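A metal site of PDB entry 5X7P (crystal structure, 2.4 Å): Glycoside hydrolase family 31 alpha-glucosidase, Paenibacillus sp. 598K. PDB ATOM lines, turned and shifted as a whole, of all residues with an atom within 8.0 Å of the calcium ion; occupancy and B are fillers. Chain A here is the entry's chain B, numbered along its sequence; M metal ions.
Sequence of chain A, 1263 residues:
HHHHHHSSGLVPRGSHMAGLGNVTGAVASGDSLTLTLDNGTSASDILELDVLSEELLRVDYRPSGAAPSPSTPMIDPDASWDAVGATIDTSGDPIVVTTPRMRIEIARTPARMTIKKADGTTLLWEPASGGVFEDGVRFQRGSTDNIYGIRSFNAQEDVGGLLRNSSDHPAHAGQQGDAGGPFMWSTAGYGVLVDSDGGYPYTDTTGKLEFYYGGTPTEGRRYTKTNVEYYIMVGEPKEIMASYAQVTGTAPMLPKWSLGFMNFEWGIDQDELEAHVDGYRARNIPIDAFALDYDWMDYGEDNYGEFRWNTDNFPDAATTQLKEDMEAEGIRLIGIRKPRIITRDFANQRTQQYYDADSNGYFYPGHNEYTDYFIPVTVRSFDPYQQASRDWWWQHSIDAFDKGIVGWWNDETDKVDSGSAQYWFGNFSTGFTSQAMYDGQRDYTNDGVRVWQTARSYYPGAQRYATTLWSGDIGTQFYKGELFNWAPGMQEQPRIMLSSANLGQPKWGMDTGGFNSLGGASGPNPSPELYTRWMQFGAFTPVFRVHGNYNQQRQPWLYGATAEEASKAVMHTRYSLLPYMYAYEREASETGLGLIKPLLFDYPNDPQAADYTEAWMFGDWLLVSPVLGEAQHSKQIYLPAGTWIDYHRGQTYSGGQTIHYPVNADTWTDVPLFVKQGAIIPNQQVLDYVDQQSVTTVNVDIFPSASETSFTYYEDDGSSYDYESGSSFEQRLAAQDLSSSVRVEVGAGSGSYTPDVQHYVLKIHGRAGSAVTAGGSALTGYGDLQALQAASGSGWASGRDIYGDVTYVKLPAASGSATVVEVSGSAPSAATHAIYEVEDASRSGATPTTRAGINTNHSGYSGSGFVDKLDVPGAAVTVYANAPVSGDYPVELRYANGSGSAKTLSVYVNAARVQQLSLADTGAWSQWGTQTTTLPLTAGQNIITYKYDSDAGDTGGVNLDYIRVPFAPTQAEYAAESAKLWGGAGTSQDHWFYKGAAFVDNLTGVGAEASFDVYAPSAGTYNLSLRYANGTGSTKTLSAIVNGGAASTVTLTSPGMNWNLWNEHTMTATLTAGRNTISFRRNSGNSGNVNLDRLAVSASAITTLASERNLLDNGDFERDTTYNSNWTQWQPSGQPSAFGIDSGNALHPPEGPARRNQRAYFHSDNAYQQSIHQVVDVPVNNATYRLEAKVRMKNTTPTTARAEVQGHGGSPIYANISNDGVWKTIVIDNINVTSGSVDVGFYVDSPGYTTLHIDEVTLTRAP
The calcium ion is bound by O of Gln 1158 (2.4 Å), O of Asp 1116 (2.4 Å), OD1 of Asp 1255 (2.4 Å), OE2 of Glu 1118 (2.4 Å), OD2 of Asp 1255 (2.7 Å) and O of Arg 1155 (2.8 Å). The calcium ion has six donor atoms within binding distance. Slightly farther from the calcium ion lies the side-chain carboxylate (OE2) of Glu 1256 (3.0 Å).
Six residues have an atom within 4 Å of the calcium ion: Asp 1116, Glu 1118, Arg 1155, Gln 1158, Asp 1255 and Glu 1256. The nearest printed residue that does not touch the calcium ion is Pro 1153 (4.5 Å).
NE2 of Gln 1158 lies within hydrogen-bond range of O of Arg 1119, 2.7 Å away. OD2 of Asp 1255 sits close to N of Ala 1154 (3.0 Å). The side-chain carboxylate of Glu 1118 is in salt-bridge range of the guanidinium group of Arg 1156, at 2.6 Å. N of Asn 1157 is in hydrogen-bond range of OE1 of Glu 1118 (3.0 Å). OD1 of Asn 1114 lies within hydrogen-bond range of N of Glu 1118 (3.1 Å). NE of Arg 1155 is in salt-bridge range of OE1 of Glu 1256, 2.6 Å away. OD1 of Asp 666 lies within salt-bridge range of NH2 of Arg 1155, at 2.8 Å. N of Glu 1256 lies within hydrogen-bond range of O of Gly 1115.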
ATOM      1  N   THR A 562       9.826  14.274  20.842  1.00  0.00           N
ATOM      2  CA  THR A 562       8.424  13.993  21.112  1.00  0.00           C
ATOM      3  C   THR A 562       8.061  12.611  20.555  1.00  0.00           C
ATOM      4  O   THR A 562       7.361  11.817  21.214  1.00  0.00           O
ATOM      5  CB  THR A 562       7.508  14.998  20.461  1.00  0.00           C
ATOM      6  OG1 THR A 562       7.842  16.288  20.951  1.00  0.00           O
ATOM      7  CG2 THR A 562       6.048  14.675  20.771  1.00  0.00           C
ATOM      8  N   ASP A 666       0.262  20.385  21.187  1.00  0.00           N
ATOM      9  CA  ASP A 666       1.645  20.770  21.332  1.00  0.00           C
ATOM     10  C   ASP A 666       2.509  19.595  21.824  1.00  0.00           C
ATOM     11  O   ASP A 666       3.643  19.405  21.391  1.00  0.00           O
ATOM     12  CB  ASP A 666       1.750  22.000  22.228  1.00  0.00           C
ATOM     13  CG  ASP A 666       3.179  22.468  22.404  1.00  0.00           C
ATOM     14  OD1 ASP A 666       3.936  22.588  21.410  1.00  0.00           O
ATOM     15  OD2 ASP A 666       3.539  22.687  23.554  1.00  0.00           O
ATOM     16  N   ASN A1114       6.948  31.709  18.693  1.00  0.00           N
ATOM     17  CA  ASN A1114       7.434  30.606  17.813  1.00  0.00           C
ATOM     18  C   ASN A1114       8.846  30.176  18.123  1.00  0.00           C
ATOM     19  O   ASN A1114       9.649  29.928  17.218  1.00  0.00           O
ATOM     20  CB  ASN A1114       7.343  31.043  16.339  1.00  0.00           C
ATOM     21  CG  ASN A1114       7.319  29.869  15.374  1.00  0.00           C
ATOM     22  OD1 ASN A1114       6.796  28.777  15.689  1.00  0.00           O
ATOM     23  ND2 ASN A1114       7.864  30.093  14.180  1.00  0.00           N
ATOM     24  N   GLY A1115       9.171  30.052  19.388  1.00  0.00           N
ATOM     25  CA  GLY A1115      10.549  29.685  19.779  1.00  0.00           C
ATOM     26  C   GLY A1115      10.928  28.276  19.414  1.00  0.00           C
ATOM     27  O   GLY A1115      12.136  27.960  19.300  1.00  0.00           O
ATOM     28  N   ASP A1116       9.883  27.427  19.245  1.00  0.00           N
ATOM     29  CA  ASP A1116      10.039  26.029  18.907  1.00  0.00           C
ATOM     30  C   ASP A1116       9.887  25.787  17.389  1.00  0.00           C
ATOM     31  O   ASP A1116      10.003  24.637  16.942  1.00  0.00           O
ATOM     32  CB  ASP A1116       9.041  25.174  19.679  1.00  0.00           C
ATOM     33  CG  ASP A1116       7.611  25.627  19.529  1.00  0.00           C
ATOM     34  OD1 ASP A1116       7.353  26.499  18.663  1.00  0.00           O
ATOM     35  OD2 ASP A1116       6.735  25.110  20.304  1.00  0.00           O
ATOM     36  N   PHE A1117       9.615  26.866  16.634  1.00  0.00           N
ATOM     37  CA  PHE A1117       9.444  26.825  15.206  1.00  0.00           C
ATOM     38  C   PHE A1117       8.301  25.925  14.718  1.00  0.00           C
ATOM     39  O   PHE A1117       8.300  25.509  13.562  1.00  0.00           O
ATOM     40  CB  PHE A1117      10.756  26.455  14.515  1.00  0.00           C
ATOM     41  CG  PHE A1117      11.899  27.357  14.864  1.00  0.00           C
ATOM     42  CD1 PHE A1117      11.965  28.638  14.309  1.00  0.00           C
ATOM     43  CD2 PHE A1117      12.866  26.965  15.766  1.00  0.00           C
ATOM     44  CE1 PHE A1117      12.991  29.484  14.655  1.00  0.00           C
ATOM     45  CE2 PHE A1117      13.900  27.793  16.087  1.00  0.00           C
ATOM     46  CZ  PHE A1117      13.964  29.057  15.547  1.00  0.00           C
ATOM     47  N   GLU A1118       7.294  25.699  15.583  1.00  0.00           N
ATOM     48  CA  GLU A1118       6.218  24.769  15.312  1.00  0.00           C
ATOM     49  C   GLU A1118       5.086  25.322  14.484  1.00  0.00           C
ATOM     50  O   GLU A1118       4.291  24.573  13.935  1.00  0.00           O
ATOM     51  CB  GLU A1118       5.668  24.205  16.628  1.00  0.00           C
ATOM     52  CG  GLU A1118       6.639  23.267  17.327  1.00  0.00           C
ATOM     53  CD  GLU A1118       7.062  22.124  16.422  1.00  0.00           C
ATOM     54  OE1 GLU A1118       6.215  21.440  15.852  1.00  0.00           O
ATOM     55  OE2 GLU A1118       8.268  21.929  16.221  1.00  0.00           O
ATOM     56  N   ARG A1119       5.012  26.625  14.357  1.00  0.00           N
ATOM     57  CA  ARG A1119       3.994  27.247  13.540  1.00  0.00           C
ATOM     58  C   ARG A1119       4.100  26.749  12.082  1.00  0.00           C
ATOM     59  O   ARG A1119       5.193  26.468  11.546  1.00  0.00           O
ATOM     60  CB  ARG A1119       4.126  28.823  13.625  1.00  0.00           C
ATOM     61  CG  ARG A1119       2.993  29.640  12.960  1.00  0.00           C
ATOM     62  CD  ARG A1119       2.906  31.107  13.425  1.00  0.00           C
ATOM     63  NE  ARG A1119       2.965  31.164  14.884  1.00  0.00           N
ATOM     64  CZ  ARG A1119       3.489  32.135  15.625  1.00  0.00           C
ATOM     65  NH1 ARG A1119       3.947  33.265  15.081  1.00  0.00           N
ATOM     66  NH2 ARG A1119       3.532  31.971  16.928  1.00  0.00           N
ATOM     67  N   ILE A1141      12.576  26.519   7.736  1.00  0.00           N
ATOM     68  CA  ILE A1141      12.022  25.630   8.745  1.00  0.00           C
ATOM     69  C   ILE A1141      11.289  24.496   8.039  1.00  0.00           C
ATOM     70  O   ILE A1141      10.441  24.747   7.173  1.00  0.00           O
ATOM     71  CB  ILE A1141      11.015  26.364   9.627  1.00  0.00           C
ATOM     72  CG1 ILE A1141      11.657  27.553  10.349  1.00  0.00           C
ATOM     73  CG2 ILE A1141      10.395  25.392  10.642  1.00  0.00           C
ATOM     74  CD1 ILE A1141      10.698  28.716  10.604  1.00  0.00           C
ATOM     75  N   ASP A1142      11.653  23.247   8.362  1.00  0.00           N
ATOM     76  CA  ASP A1142      10.816  22.083   8.043  1.00  0.00           C
ATOM     77  C   ASP A1142      11.187  20.973   9.013  1.00  0.00           C
ATOM     78  O   ASP A1142      11.783  21.269  10.040  1.00  0.00           O
ATOM     79  CB  ASP A1142      10.919  21.671   6.561  1.00  0.00           C
ATOM     80  CG  ASP A1142      12.334  21.551   6.083  1.00  0.00           C
ATOM     81  OD1 ASP A1142      13.098  20.746   6.684  1.00  0.00           O
ATOM     82  OD2 ASP A1142      12.667  22.279   5.116  1.00  0.00           O
ATOM     83  N   GLY A1152      15.941  15.005  12.395  1.00  0.00           N
ATOM     84  CA  GLY A1152      14.673  15.461  12.946  1.00  0.00           C
ATOM     85  C   GLY A1152      14.720  16.794  13.694  1.00  0.00           C
ATOM     86  O   GLY A1152      15.694  17.543  13.627  1.00  0.00           O
ATOM     87  N   PRO A1153      13.611  17.105  14.377  1.00  0.00           N
ATOM     88  CA  PRO A1153      13.555  18.245  15.301  1.00  0.00           C
ATOM     89  C   PRO A1153      14.018  17.831  16.669  1.00  0.00           C
ATOM     90  O   PRO A1153      14.151  16.623  16.902  1.00  0.00           O
ATOM     91  CB  PRO A1153      12.070  18.603  15.302  1.00  0.00           C
ATOM     92  CG  PRO A1153      11.368  17.326  14.973  1.00  0.00           C
ATOM     93  CD  PRO A1153      12.286  16.521  14.109  1.00  0.00           C
ATOM     94  N   ALA A1154      14.317  18.783  17.551  1.00  0.00           N
ATOM     95  CA  ALA A1154      14.577  18.459  18.962  1.00  0.00           C
ATOM     96  C   ALA A1154      13.285  18.025  19.674  1.00  0.00           C
ATOM     97  O   ALA A1154      13.276  17.016  20.414  1.00  0.00           O
ATOM     98  CB  ALA A1154      15.216  19.623  19.711  1.00  0.00           C
ATOM     99  N   ARG A1155      12.225  18.790  19.447  1.00  0.00           N
ATOM    100  CA  ARG A1155      10.904  18.526  19.988  1.00  0.00           C
ATOM    101  C   ARG A1155       9.855  18.688  18.904  1.00  0.00           C
ATOM    102  O   ARG A1155       9.975  19.553  18.006  1.00  0.00           O
ATOM    103  CB  ARG A1155      10.557  19.479  21.135  1.00  0.00           C
ATOM    104  CG  ARG A1155       9.516  18.930  22.111  1.00  0.00           C
ATOM    105  CD  ARG A1155       9.095  19.909  23.211  1.00  0.00           C
ATOM    106  NE  ARG A1155       8.392  21.018  22.575  1.00  0.00           N
ATOM    107  CZ  ARG A1155       7.126  20.998  22.126  1.00  0.00           C
ATOM    108  NH1 ARG A1155       6.340  19.915  22.277  1.00  0.00           N
ATOM    109  NH2 ARG A1155       6.652  22.085  21.531  1.00  0.00           N
ATOM    110  N   ARG A1156       8.818  17.874  19.005  1.00  0.00           N
ATOM    111  CA  ARG A1156       7.643  17.998  18.135  1.00  0.00           C
ATOM    112  C   ARG A1156       7.983  17.812  16.650  1.00  0.00           C
ATOM    113  O   ARG A1156       8.635  16.815  16.316  1.00  0.00           O
ATOM    114  CB  ARG A1156       6.884  19.281  18.460  1.00  0.00           C
ATOM    115  CG  ARG A1156       5.451  19.229  17.989  1.00  0.00           C
ATOM    116  CD  ARG A1156       4.597  20.349  18.527  1.00  0.00           C
ATOM    117  NE  ARG A1156       3.237  20.184  18.051  1.00  0.00           N
ATOM    118  CZ  ARG A1156       2.819  20.575  16.860  1.00  0.00           C
ATOM    119  NH1 ARG A1156       3.618  21.186  16.019  1.00  0.00           N
ATOM    120  NH2 ARG A1156       1.560  20.345  16.512  1.00  0.00           N
ATOM    121  N   ASN A1157       7.589  18.747  15.765  1.00  0.00           N
ATOM    122  CA  ASN A1157       7.526  18.486  14.317  1.00  0.00           C
ATOM    123  C   ASN A1157       8.538  19.249  13.478  1.00  0.00           C
ATOM    124  O   ASN A1157       8.874  18.801  12.394  1.00  0.00           O
ATOM    125  CB  ASN A1157       6.115  18.828  13.766  1.00  0.00           C
ATOM    126  CG  ASN A1157       5.731  18.010  12.517  1.00  0.00           C
ATOM    127  OD1 ASN A1157       6.066  16.831  12.388  1.00  0.00           O
ATOM    128  ND2 ASN A1157       5.031  18.647  11.605  1.00  0.00           N
ATOM    129  N   GLN A1158       9.032  20.378  13.966  1.00  0.00           N
ATOM    130  CA  GLN A1158       9.748  21.321  13.132  1.00  0.00           C
ATOM    131  C   GLN A1158      11.019  21.852  13.848  1.00  0.00           C
ATOM    132  O   GLN A1158      11.091  21.924  15.104  1.00  0.00           O
ATOM    133  CB  GLN A1158       8.790  22.468  12.698  1.00  0.00           C
ATOM    134  CG  GLN A1158       8.035  22.140  11.427  1.00  0.00           C
ATOM    135  CD  GLN A1158       6.944  23.133  11.013  1.00  0.00           C
ATOM    136  OE1 GLN A1158       6.262  22.887  10.025  1.00  0.00           O
ATOM    137  NE2 GLN A1158       6.768  24.246  11.743  1.00  0.00           N
ATOM    138  N   ARG A1159      12.018  22.221  13.049  1.00  0.00           N
ATOM    139  CA  ARG A1159      13.234  22.867  13.550  1.00  0.00           C
ATOM    140  C   ARG A1159      13.774  23.794  12.495  1.00  0.00           C
ATOM    141  O   ARG A1159      13.606  23.524  11.290  1.00  0.00           O
ATOM    142  CB  ARG A1159      14.280  21.859  13.989  1.00  0.00           C
ATOM    143  CG  ARG A1159      15.036  21.159  12.886  1.00  0.00           C
ATOM    144  CD  ARG A1159      14.214  20.119  12.121  1.00  0.00           C
ATOM    145  NE  ARG A1159      15.091  19.350  11.238  1.00  0.00           N
ATOM    146  CZ  ARG A1159      15.587  19.780  10.083  1.00  0.00           C
ATOM    147  NH1 ARG A1159      15.272  20.996   9.600  1.00  0.00           N
ATOM    148  NH2 ARG A1159      16.403  18.990   9.393  1.00  0.00           N
ATOM    149  N   ALA A1160      14.369  24.923  12.901  1.00  0.00           N
ATOM    150  CA  ALA A1160      14.949  25.827  11.906  1.00  0.00           C
ATOM    151  C   ALA A1160      16.244  25.217  11.435  1.00  0.00           C
ATOM    152  O   ALA A1160      16.886  24.482  12.189  1.00  0.00           O
ATOM    153  CB  ALA A1160      15.164  27.209  12.479  1.00  0.00           C
ATOM    154  N   TRP A1223      22.282  16.867  18.865  1.00  0.00           N
ATOM    155  CA  TRP A1223      21.521  17.875  19.584  1.00  0.00           C
ATOM    156  C   TRP A1223      22.219  18.179  20.891  1.00  0.00           C
ATOM    157  O   TRP A1223      22.588  17.268  21.603  1.00  0.00           O
ATOM    158  CB  TRP A1223      20.093  17.391  19.871  1.00  0.00           C
ATOM    159  CG  TRP A1223      19.152  17.568  18.714  1.00  0.00           C
ATOM    160  CD1 TRP A1223      18.490  16.589  18.037  1.00  0.00           C
ATOM    161  CD2 TRP A1223      18.763  18.814  18.087  1.00  0.00           C
ATOM    162  NE1 TRP A1223      17.714  17.139  17.044  1.00  0.00           N
ATOM    163  CE2 TRP A1223      17.886  18.503  17.036  1.00  0.00           C
ATOM    164  CE3 TRP A1223      19.092  20.162  18.304  1.00  0.00           C
ATOM    165  CZ2 TRP A1223      17.315  19.476  16.235  1.00  0.00           C
ATOM    166  CZ3 TRP A1223      18.519  21.138  17.512  1.00  0.00           C
ATOM    167  CH2 TRP A1223      17.650  20.802  16.481  1.00  0.00           C
ATOM    168  N   ILE A1254      18.387  24.578  14.818  1.00  0.00           N
ATOM    169  CA  ILE A1254      18.056  25.264  16.010  1.00  0.00           C
ATOM    170  C   ILE A1254      16.606  24.887  16.347  1.00  0.00           C
ATOM    171  O   ILE A1254      15.730  24.887  15.479  1.00  0.00           O
ATOM    172  CB  ILE A1254      18.145  26.777  15.802  1.00  0.00           C
ATOM    173  CG1 ILE A1254      19.480  27.166  15.145  1.00  0.00           C
ATOM    174  CG2 ILE A1254      18.017  27.479  17.136  1.00  0.00           C
ATOM    175  CD1 ILE A1254      19.406  28.436  14.345  1.00  0.00           C
ATOM    176  N   ASP A1255      16.363  24.577  17.607  1.00  0.00           N
ATOM    177  CA  ASP A1255      15.024  24.297  18.095  1.00  0.00           C
ATOM    178  C   ASP A1255      14.787  24.649  19.603  1.00  0.00           C
ATOM    179  O   ASP A1255      15.739  24.777  20.403  1.00  0.00           O
ATOM    180  CB  ASP A1255      14.730  22.811  17.828  1.00  0.00           C
ATOM    181  CG  ASP A1255      13.283  22.548  17.645  1.00  0.00           C
ATOM    182  OD1 ASP A1255      12.473  23.508  17.641  1.00  0.00           O
ATOM    183  OD2 ASP A1255      12.911  21.393  17.493  1.00  0.00           O
ATOM    184  N   GLU A1256      13.524  24.837  19.972  1.00  0.00           N
ATOM    185  CA  GLU A1256      13.098  24.944  21.372  1.00  0.00           C
ATOM    186  C   GLU A1256      13.785  26.083  22.097  1.00  0.00           C
ATOM    187  O   GLU A1256      14.285  25.936  23.189  1.00  0.00           O
ATOM    188  CB  GLU A1256      13.306  23.608  22.106  1.00  0.00           C
ATOM    189  CG  GLU A1256      12.625  22.427  21.415  1.00  0.00           C
ATOM    190  CD  GLU A1256      11.098  22.568  21.422  1.00  0.00           C
ATOM    191  OE1 GLU A1256      10.551  22.541  22.540  1.00  0.00           O
ATOM    192  OE2 GLU A1256      10.465  22.691  20.335  1.00  0.00           O
ATOM    193  N   VAL A1257      13.758  27.243  21.456  1.00  0.00           N
ATOM    194  CA  VAL A1257      14.422  28.402  21.999  1.00  0.00           C
ATOM    195  C   VAL A1257      13.472  28.932  23.036  1.00  0.00           C
ATOM    196  O   VAL A1257      12.256  29.027  22.771  1.00  0.00           O
ATOM    197  CB  VAL A1257      14.711  29.458  20.911  1.00  0.00           C
ATOM    198  CG1 VAL A1257      15.607  30.562  21.453  1.00  0.00           C
ATOM    199  CG2 VAL A1257      15.361  28.818  19.701  1.00  0.00           C
HETATM  200 CA    CA M   1      10.403  22.278  17.341  1.00  0.00          CA
